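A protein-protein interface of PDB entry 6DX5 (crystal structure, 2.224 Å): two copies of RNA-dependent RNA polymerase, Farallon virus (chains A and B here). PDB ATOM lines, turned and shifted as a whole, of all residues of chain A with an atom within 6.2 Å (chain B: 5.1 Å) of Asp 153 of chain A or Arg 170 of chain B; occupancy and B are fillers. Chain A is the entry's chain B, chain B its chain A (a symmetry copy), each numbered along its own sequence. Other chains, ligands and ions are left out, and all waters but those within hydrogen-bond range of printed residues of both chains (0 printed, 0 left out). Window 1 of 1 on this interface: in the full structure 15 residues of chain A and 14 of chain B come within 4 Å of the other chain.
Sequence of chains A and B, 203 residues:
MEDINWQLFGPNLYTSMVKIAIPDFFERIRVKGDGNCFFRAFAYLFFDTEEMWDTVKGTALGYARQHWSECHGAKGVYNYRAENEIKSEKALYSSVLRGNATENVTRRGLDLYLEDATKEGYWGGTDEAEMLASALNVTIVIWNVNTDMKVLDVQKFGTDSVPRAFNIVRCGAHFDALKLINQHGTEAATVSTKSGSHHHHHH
Of the 13 printed residues of chain A, 3 touch a printed residue of chain B. Hydrophobic or aromatic side chains of chain A that line the printed part of chain B: Met 17 and Leu 152. Hydrophobic or aromatic side chains of chain B that line the printed part of chain A: Ala 173. Among the printed residues, Asp or Glu carboxylates within 4 Å of a Lys or Arg side-chain nitrogen of the other chain: Asp 153 of chain A with Arg 170 of chain B (3.0 Å).
The guanidinium group (NH1) of Arg 170 of chain B lies within salt-bridge range of the side-chain carboxylate (OD1) of Asp 153 of chain A.
CE of Met 17 of chain A touches CB of Ala 173 of chain B, 3.7 Å away. CD2 of Leu 152 of chain A touches SG of Cys 171 of chain B, at 3.7 Å. O of Leu 152 of chain A touches CA of Gly 172 of chain B, 3.4 Å away. Asp 153 of chain A touches Gly 172 of chain B.
Positions printed for both chains: 142, 143, 144 and 145.
Arg 170 of chain B touches just one residue of chain A: Asp 153. Printed residues of chain B within 4 Å of Leu 152 of chain A: Cys 171 and Gly 172. Printed residues of chain A within 4 Å of Ala 173 of chain B: Met 17 (3.7 Å). Of the printed residues of chain B, Met 17 of chain A touches Ala 173 (3.7 Å). Thr 15 of chain A touches none of the printed residues of chain B. The nearest residue of chain B that does not touch Asp 153 of chain A is Ala 173 of chain B (4.5 Å).
The side-chain carboxylate of Asp 153 of chain A is in hydrogen-bond range of the side-chain amide nitrogen of Gln 155 of chain A, 3.3 Å away. The backbone NH (N) of Leu 152 of chain A is in hydrogen-bond range of the backbone carbonyl oxygen (O) of Asn 144 of chain A (2.7 Å). NH1 of Arg 170 of chain B is in hydrogen-bond range of O of Gly 172 of chain B (2.8 Å). N of Asn 144 of chain A lies within hydrogen-bond range of O of Asp 153 of chain A, at 3.0 Å. The backbone NH (N) of Val 145 of chain B is in hydrogen-bond range of the backbone carbonyl oxygen (O) of Arg 170 of chain B (2.9 Å). O of Trp 143 of chain B sits at hydrogen-bond distance from N of Arg 170 of chain B, at 2.7 Å.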
ATOM      1  N   THR A  15     -27.399 -18.149   7.625  1.00  0.00           N
ATOM      2  CA  THR A  15     -27.085 -17.531   8.888  1.00  0.00           C
ATOM      3  C   THR A  15     -25.755 -18.093   9.366  1.00  0.00           C
ATOM      4  O   THR A  15     -25.271 -19.119   8.869  1.00  0.00           O
ATOM      5  CB  THR A  15     -28.203 -17.773   9.916  1.00  0.00           C
ATOM      6  OG1 THR A  15     -27.863 -17.132  11.157  1.00  0.00           O
ATOM      7  CG2 THR A  15     -28.423 -19.277  10.142  1.00  0.00           C
ATOM      8  N   SER A  16     -25.159 -17.377  10.314  1.00  0.00           N
ATOM      9  CA  SER A  16     -23.885 -17.758  10.882  1.00  0.00           C
ATOM     10  C   SER A  16     -23.753 -17.127  12.265  1.00  0.00           C
ATOM     11  O   SER A  16     -24.267 -16.033  12.531  1.00  0.00           O
ATOM     12  CB  SER A  16     -22.735 -17.335   9.968  1.00  0.00           C
ATOM     13  OG  SER A  16     -21.530 -17.937  10.406  1.00  0.00           O
ATOM     14  N   MET A  17     -23.069 -17.844  13.148  1.00  0.00           N
ATOM     15  CA  MET A  17     -22.768 -17.340  14.476  1.00  0.00           C
ATOM     16  C   MET A  17     -21.314 -16.907  14.602  1.00  0.00           C
ATOM     17  O   MET A  17     -20.777 -16.851  15.709  1.00  0.00           O
ATOM     18  CB  MET A  17     -23.139 -18.382  15.535  1.00  0.00           C
ATOM     19  CG  MET A  17     -23.184 -19.834  15.058  1.00  0.00           C
ATOM     20  SD  MET A  17     -23.991 -20.924  16.284  1.00  0.00           S
ATOM     21  CE  MET A  17     -25.720 -20.604  15.950  1.00  0.00           C
ATOM     22  N   VAL A  18     -20.674 -16.597  13.477  1.00  0.00           N
ATOM     23  CA  VAL A  18     -19.362 -15.988  13.505  1.00  0.00           C
ATOM     24  C   VAL A  18     -19.452 -14.652  14.243  1.00  0.00           C
ATOM     25  O   VAL A  18     -20.370 -13.851  14.020  1.00  0.00           O
ATOM     26  CB  VAL A  18     -18.821 -15.824  12.070  1.00  0.00           C
ATOM     27  CG1 VAL A  18     -19.696 -14.834  11.199  1.00  0.00           C
ATOM     28  CG2 VAL A  18     -17.351 -15.398  12.107  1.00  0.00           C
ATOM     29  N   ILE A 142     -26.556  -8.989   6.140  1.00  0.00           N
ATOM     30  CA  ILE A 142     -27.075  -8.101   7.178  1.00  0.00           C
ATOM     31  C   ILE A 142     -26.354  -8.456   8.471  1.00  0.00           C
ATOM     32  O   ILE A 142     -26.506  -9.566   8.989  1.00  0.00           O
ATOM     33  CB  ILE A 142     -28.587  -8.232   7.381  1.00  0.00           C
ATOM     34  CG1 ILE A 142     -29.364  -8.166   6.056  1.00  0.00           C
ATOM     35  CG2 ILE A 142     -29.056  -7.143   8.372  1.00  0.00           C
ATOM     36  CD1 ILE A 142     -29.456  -6.819   5.512  1.00  0.00           C
ATOM     37  N   TRP A 143     -25.572  -7.532   9.002  1.00  0.00           N
ATOM     38  CA  TRP A 143     -24.852  -7.761  10.250  1.00  0.00           C
ATOM     39  C   TRP A 143     -25.618  -7.045  11.361  1.00  0.00           C
ATOM     40  O   TRP A 143     -25.726  -5.814  11.352  1.00  0.00           O
ATOM     41  CB  TRP A 143     -23.411  -7.226  10.178  1.00  0.00           C
ATOM     42  CG  TRP A 143     -22.551  -7.766   9.086  1.00  0.00           C
ATOM     43  CD1 TRP A 143     -22.525  -7.351   7.785  1.00  0.00           C
ATOM     44  CD2 TRP A 143     -21.633  -8.866   9.184  1.00  0.00           C
ATOM     45  NE1 TRP A 143     -21.623  -8.103   7.070  1.00  0.00           N
ATOM     46  CE2 TRP A 143     -21.069  -9.043   7.904  1.00  0.00           C
ATOM     47  CE3 TRP A 143     -21.224  -9.704  10.233  1.00  0.00           C
ATOM     48  CZ2 TRP A 143     -20.117 -10.048   7.624  1.00  0.00           C
ATOM     49  CZ3 TRP A 143     -20.255 -10.696   9.964  1.00  0.00           C
ATOM     50  CH2 TRP A 143     -19.746 -10.875   8.663  1.00  0.00           C
ATOM     51  N   ASN A 144     -26.152  -7.800  12.303  1.00  0.00           N
ATOM     52  CA  ASN A 144     -26.853  -7.202  13.421  1.00  0.00           C
ATOM     53  C   ASN A 144     -25.838  -6.959  14.529  1.00  0.00           C
ATOM     54  O   ASN A 144     -25.215  -7.909  15.027  1.00  0.00           O
ATOM     55  CB  ASN A 144     -27.980  -8.126  13.903  1.00  0.00           C
ATOM     56  CG  ASN A 144     -28.943  -8.493  12.788  1.00  0.00           C
ATOM     57  OD1 ASN A 144     -28.939  -9.632  12.289  1.00  0.00           O
ATOM     58  ND2 ASN A 144     -29.702  -7.524  12.335  1.00  0.00           N
ATOM     59  N   VAL A 145     -25.711  -5.721  14.965  1.00  0.00           N
ATOM     60  CA  VAL A 145     -24.688  -5.399  15.940  1.00  0.00           C
ATOM     61  C   VAL A 145     -25.305  -4.733  17.158  1.00  0.00           C
ATOM     62  O   VAL A 145     -26.423  -4.205  17.120  1.00  0.00           O
ATOM     63  CB  VAL A 145     -23.635  -4.496  15.320  1.00  0.00           C
ATOM     64  CG1 VAL A 145     -23.019  -5.175  14.114  1.00  0.00           C
ATOM     65  CG2 VAL A 145     -24.292  -3.139  14.991  1.00  0.00           C
ATOM     66  N   VAL A 151     -20.756  -7.911  16.726  1.00  0.00           N
ATOM     67  CA  VAL A 151     -21.789  -8.638  15.999  1.00  0.00           C
ATOM     68  C   VAL A 151     -22.602  -9.501  16.954  1.00  0.00           C
ATOM     69  O   VAL A 151     -22.045 -10.222  17.799  1.00  0.00           O
ATOM     70  CB  VAL A 151     -21.162  -9.499  14.893  1.00  0.00           C
ATOM     71  CG1 VAL A 151     -22.253 -10.310  14.170  1.00  0.00           C
ATOM     72  CG2 VAL A 151     -20.455  -8.632  13.898  1.00  0.00           C
ATOM     73  N   LEU A 152     -23.933  -9.441  16.829  1.00  0.00           N
ATOM     74  CA  LEU A 152     -24.789 -10.379  17.559  1.00  0.00           C
ATOM     75  C   LEU A 152     -25.077 -11.610  16.698  1.00  0.00           C
ATOM     76  O   LEU A 152     -24.953 -12.735  17.170  1.00  0.00           O
ATOM     77  CB  LEU A 152     -26.112  -9.710  17.970  1.00  0.00           C
ATOM     78  CG  LEU A 152     -26.098  -8.469  18.862  1.00  0.00           C
ATOM     79  CD1 LEU A 152     -27.335  -7.566  18.659  1.00  0.00           C
ATOM     80  CD2 LEU A 152     -26.060  -8.960  20.257  1.00  0.00           C
ATOM     81  N   ASP A 153     -25.492 -11.406  15.449  1.00  0.00           N
ATOM     82  CA  ASP A 153     -25.583 -12.499  14.485  1.00  0.00           C
ATOM     83  C   ASP A 153     -25.676 -11.867  13.107  1.00  0.00           C
ATOM     84  O   ASP A 153     -25.684 -10.638  12.967  1.00  0.00           O
ATOM     85  CB  ASP A 153     -26.758 -13.444  14.778  1.00  0.00           C
ATOM     86  CG  ASP A 153     -28.058 -12.699  15.029  1.00  0.00           C
ATOM     87  OD1 ASP A 153     -28.640 -12.825  16.145  1.00  0.00           O
ATOM     88  OD2 ASP A 153     -28.481 -11.963  14.103  1.00  0.00           O
ATOM     89  N   VAL A 154     -25.695 -12.714  12.075  1.00  0.00           N
ATOM     90  CA  VAL A 154     -25.603 -12.214  10.711  1.00  0.00           C
ATOM     91  C   VAL A 154     -26.361 -13.163   9.796  1.00  0.00           C
ATOM     92  O   VAL A 154     -26.320 -14.375   9.995  1.00  0.00           O
ATOM     93  CB  VAL A 154     -24.127 -12.041  10.294  1.00  0.00           C
ATOM     94  CG1 VAL A 154     -23.385 -13.302  10.513  1.00  0.00           C
ATOM     95  CG2 VAL A 154     -24.013 -11.589   8.856  1.00  0.00           C
ATOM     96  N   GLN A 155     -27.121 -12.593   8.843  1.00  0.00           N
ATOM     97  CA  GLN A 155     -27.828 -13.299   7.788  1.00  0.00           C
ATOM     98  C   GLN A 155     -27.293 -12.840   6.442  1.00  0.00           C
ATOM     99  O   GLN A 155     -26.793 -11.706   6.283  1.00  0.00           O
ATOM    100  CB  GLN A 155     -29.330 -13.038   7.800  1.00  0.00           C
ATOM    101  CG  GLN A 155     -30.019 -13.286   9.076  1.00  0.00           C
ATOM    102  CD  GLN A 155     -30.304 -11.988   9.837  1.00  0.00           C
ATOM    103  OE1 GLN A 155     -31.067 -11.086   9.365  1.00  0.00           O
ATOM    104  NE2 GLN A 155     -29.680 -11.872  11.017  1.00  0.00           N
ATOM    105  N   ILE B 142     -40.740 -14.626  22.593  1.00  0.00           N
ATOM    106  CA  ILE B 142     -39.297 -14.559  22.381  1.00  0.00           C
ATOM    107  C   ILE B 142     -38.898 -13.120  22.205  1.00  0.00           C
ATOM    108  O   ILE B 142     -39.199 -12.510  21.175  1.00  0.00           O
ATOM    109  CB  ILE B 142     -38.847 -15.381  21.189  1.00  0.00           C
ATOM    110  CG1 ILE B 142     -39.424 -16.799  21.390  1.00  0.00           C
ATOM    111  CG2 ILE B 142     -37.296 -15.316  21.089  1.00  0.00           C
ATOM    112  CD1 ILE B 142     -38.773 -17.791  20.633  1.00  0.00           C
ATOM    113  N   TRP B 143     -38.207 -12.587  23.214  1.00  0.00           N
ATOM    114  CA  TRP B 143     -37.655 -11.240  23.212  1.00  0.00           C
ATOM    115  C   TRP B 143     -36.231 -11.285  22.648  1.00  0.00           C
ATOM    116  O   TRP B 143     -35.350 -11.923  23.227  1.00  0.00           O
ATOM    117  CB  TRP B 143     -37.658 -10.694  24.649  1.00  0.00           C
ATOM    118  CG  TRP B 143     -39.005 -10.693  25.395  1.00  0.00           C
ATOM    119  CD1 TRP B 143     -39.599 -11.737  26.132  1.00  0.00           C
ATOM    120  CD2 TRP B 143     -39.909  -9.579  25.464  1.00  0.00           C
ATOM    121  NE1 TRP B 143     -40.832 -11.293  26.648  1.00  0.00           N
ATOM    122  CE2 TRP B 143     -41.030  -9.985  26.250  1.00  0.00           C
ATOM    123  CE3 TRP B 143     -39.866  -8.265  24.957  1.00  0.00           C
ATOM    124  CZ2 TRP B 143     -42.078  -9.115  26.537  1.00  0.00           C
ATOM    125  CZ3 TRP B 143     -40.918  -7.418  25.220  1.00  0.00           C
ATOM    126  CH2 TRP B 143     -42.011  -7.845  25.998  1.00  0.00           C
ATOM    127  N   ASN B 144     -36.002 -10.625  21.532  1.00  0.00           N
ATOM    128  CA  ASN B 144     -34.679 -10.519  20.944  1.00  0.00           C
ATOM    129  C   ASN B 144     -34.035  -9.216  21.417  1.00  0.00           C
ATOM    130  O   ASN B 144     -34.618  -8.145  21.242  1.00  0.00           O
ATOM    131  CB  ASN B 144     -34.812 -10.561  19.426  1.00  0.00           C
ATOM    132  CG  ASN B 144     -33.484 -10.421  18.733  1.00  0.00           C
ATOM    133  OD1 ASN B 144     -33.379  -9.764  17.685  1.00  0.00           O
ATOM    134  ND2 ASN B 144     -32.456 -11.009  19.317  1.00  0.00           N
ATOM    135  N   VAL B 145     -32.878  -9.308  22.076  1.00  0.00           N
ATOM    136  CA  VAL B 145     -32.264  -8.162  22.743  1.00  0.00           C
ATOM    137  C   VAL B 145     -30.827  -8.008  22.281  1.00  0.00           C
ATOM    138  O   VAL B 145     -30.241  -8.913  21.682  1.00  0.00           O
ATOM    139  CB  VAL B 145     -32.276  -8.301  24.279  1.00  0.00           C
ATOM    140  CG1 VAL B 145     -33.692  -8.406  24.827  1.00  0.00           C
ATOM    141  CG2 VAL B 145     -31.381  -9.486  24.700  1.00  0.00           C
ATOM    142  N   ILE B 168     -38.931 -16.017  27.011  1.00  0.00           N
ATOM    143  CA  ILE B 168     -37.580 -16.459  26.654  1.00  0.00           C
ATOM    144  C   ILE B 168     -36.839 -15.242  26.110  1.00  0.00           C
ATOM    145  O   ILE B 168     -37.451 -14.416  25.437  1.00  0.00           O
ATOM    146  CB  ILE B 168     -37.656 -17.561  25.566  1.00  0.00           C
ATOM    147  CG1 ILE B 168     -38.452 -18.784  26.037  1.00  0.00           C
ATOM    148  CG2 ILE B 168     -36.300 -17.984  25.058  1.00  0.00           C
ATOM    149  CD1 ILE B 168     -37.985 -19.281  27.261  1.00  0.00           C
ATOM    150  N   VAL B 169     -35.537 -15.109  26.359  1.00  0.00           N
ATOM    151  CA  VAL B 169     -34.788 -13.985  25.792  1.00  0.00           C
ATOM    152  C   VAL B 169     -33.746 -14.542  24.829  1.00  0.00           C
ATOM    153  O   VAL B 169     -33.105 -15.566  25.114  1.00  0.00           O
ATOM    154  CB  VAL B 169     -34.170 -13.106  26.902  1.00  0.00           C
ATOM    155  CG1 VAL B 169     -33.227 -13.896  27.823  1.00  0.00           C
ATOM    156  CG2 VAL B 169     -33.460 -11.919  26.311  1.00  0.00           C
ATOM    157  N   ARG B 170     -33.620 -13.927  23.663  1.00  0.00           N
ATOM    158  CA  ARG B 170     -32.579 -14.308  22.715  1.00  0.00           C
ATOM    159  C   ARG B 170     -31.579 -13.166  22.606  1.00  0.00           C
ATOM    160  O   ARG B 170     -31.974 -12.001  22.433  1.00  0.00           O
ATOM    161  CB  ARG B 170     -33.162 -14.629  21.323  1.00  0.00           C
ATOM    162  CG  ARG B 170     -32.109 -15.078  20.351  1.00  0.00           C
ATOM    163  CD  ARG B 170     -32.683 -15.554  19.015  1.00  0.00           C
ATOM    164  NE  ARG B 170     -33.209 -14.496  18.175  1.00  0.00           N
ATOM    165  CZ  ARG B 170     -32.485 -13.703  17.374  1.00  0.00           C
ATOM    166  NH1 ARG B 170     -31.161 -13.802  17.338  1.00  0.00           N
ATOM    167  NH2 ARG B 170     -33.087 -12.795  16.590  1.00  0.00           N
ATOM    168  N   CYS B 171     -30.282 -13.493  22.694  1.00  0.00           N
ATOM    169  CA  CYS B 171     -29.226 -12.516  22.429  1.00  0.00           C
ATOM    170  C   CYS B 171     -28.280 -13.174  21.434  1.00  0.00           C
ATOM    171  O   CYS B 171     -27.487 -14.054  21.801  1.00  0.00           O
ATOM    172  CB  CYS B 171     -28.493 -12.071  23.707  1.00  0.00           C
ATOM    173  SG  CYS B 171     -27.184 -10.778  23.321  1.00  0.00           S
ATOM    174  N   GLY B 172     -28.386 -12.772  20.166  1.00  0.00           N
ATOM    175  CA  GLY B 172     -27.650 -13.461  19.119  1.00  0.00           C
ATOM    176  C   GLY B 172     -28.105 -14.906  19.048  1.00  0.00           C
ATOM    177  O   GLY B 172     -29.290 -15.216  18.897  1.00  0.00           O
ATOM    178  N   ALA B 173     -27.188 -15.835  19.198  1.00  0.00           N
ATOM    179  CA  ALA B 173     -27.585 -17.229  19.078  1.00  0.00           C
ATOM    180  C   ALA B 173     -28.025 -17.846  20.399  1.00  0.00           C
ATOM    181  O   ALA B 173     -28.452 -19.000  20.405  1.00  0.00           O
ATOM    182  CB  ALA B 173     -26.426 -18.039  18.498  1.00  0.00           C
ATOM    183  N   HIS B 174     -27.949 -17.122  21.515  1.00  0.00           N
ATOM    184  CA  HIS B 174     -28.108 -17.749  22.814  1.00  0.00           C
ATOM    185  C   HIS B 174     -29.470 -17.386  23.420  1.00  0.00           C
ATOM    186  O   HIS B 174     -29.839 -16.211  23.467  1.00  0.00           O
ATOM    187  CB  HIS B 174     -26.939 -17.345  23.748  1.00  0.00           C
ATOM    188  CG  HIS B 174     -27.070 -17.937  25.116  1.00  0.00           C
ATOM    189  ND1 HIS B 174     -26.894 -19.287  25.360  1.00  0.00           N
ATOM    190  CD2 HIS B 174     -27.495 -17.392  26.288  1.00  0.00           C
ATOM    191  CE1 HIS B 174     -27.145 -19.536  26.638  1.00  0.00           C
ATOM    192  NE2 HIS B 174     -27.522 -18.406  27.220  1.00  0.00           N
ATOM    193  N   PHE B 175     -30.193 -18.387  23.932  1.00  0.00           N
ATOM    194  CA  PHE B 175     -31.462 -18.174  24.617  1.00  0.00           C
ATOM    195  C   PHE B 175     -31.286 -18.368  26.121  1.00  0.00           C
ATOM    196  O   PHE B 175     -30.563 -19.279  26.536  1.00  0.00           O
ATOM    197  CB  PHE B 175     -32.518 -19.170  24.145  1.00  0.00           C
ATOM    198  CG  PHE B 175     -32.860 -19.077  22.671  1.00  0.00           C
ATOM    199  CD1 PHE B 175     -33.974 -18.355  22.253  1.00  0.00           C
ATOM    200  CD2 PHE B 175     -32.055 -19.714  21.720  1.00  0.00           C
ATOM    201  CE1 PHE B 175     -34.303 -18.270  20.897  1.00  0.00           C
ATOM    202  CE2 PHE B 175     -32.371 -19.645  20.380  1.00  0.00           C
ATOM    203  CZ  PHE B 175     -33.492 -18.915  19.954  1.00  0.00           C
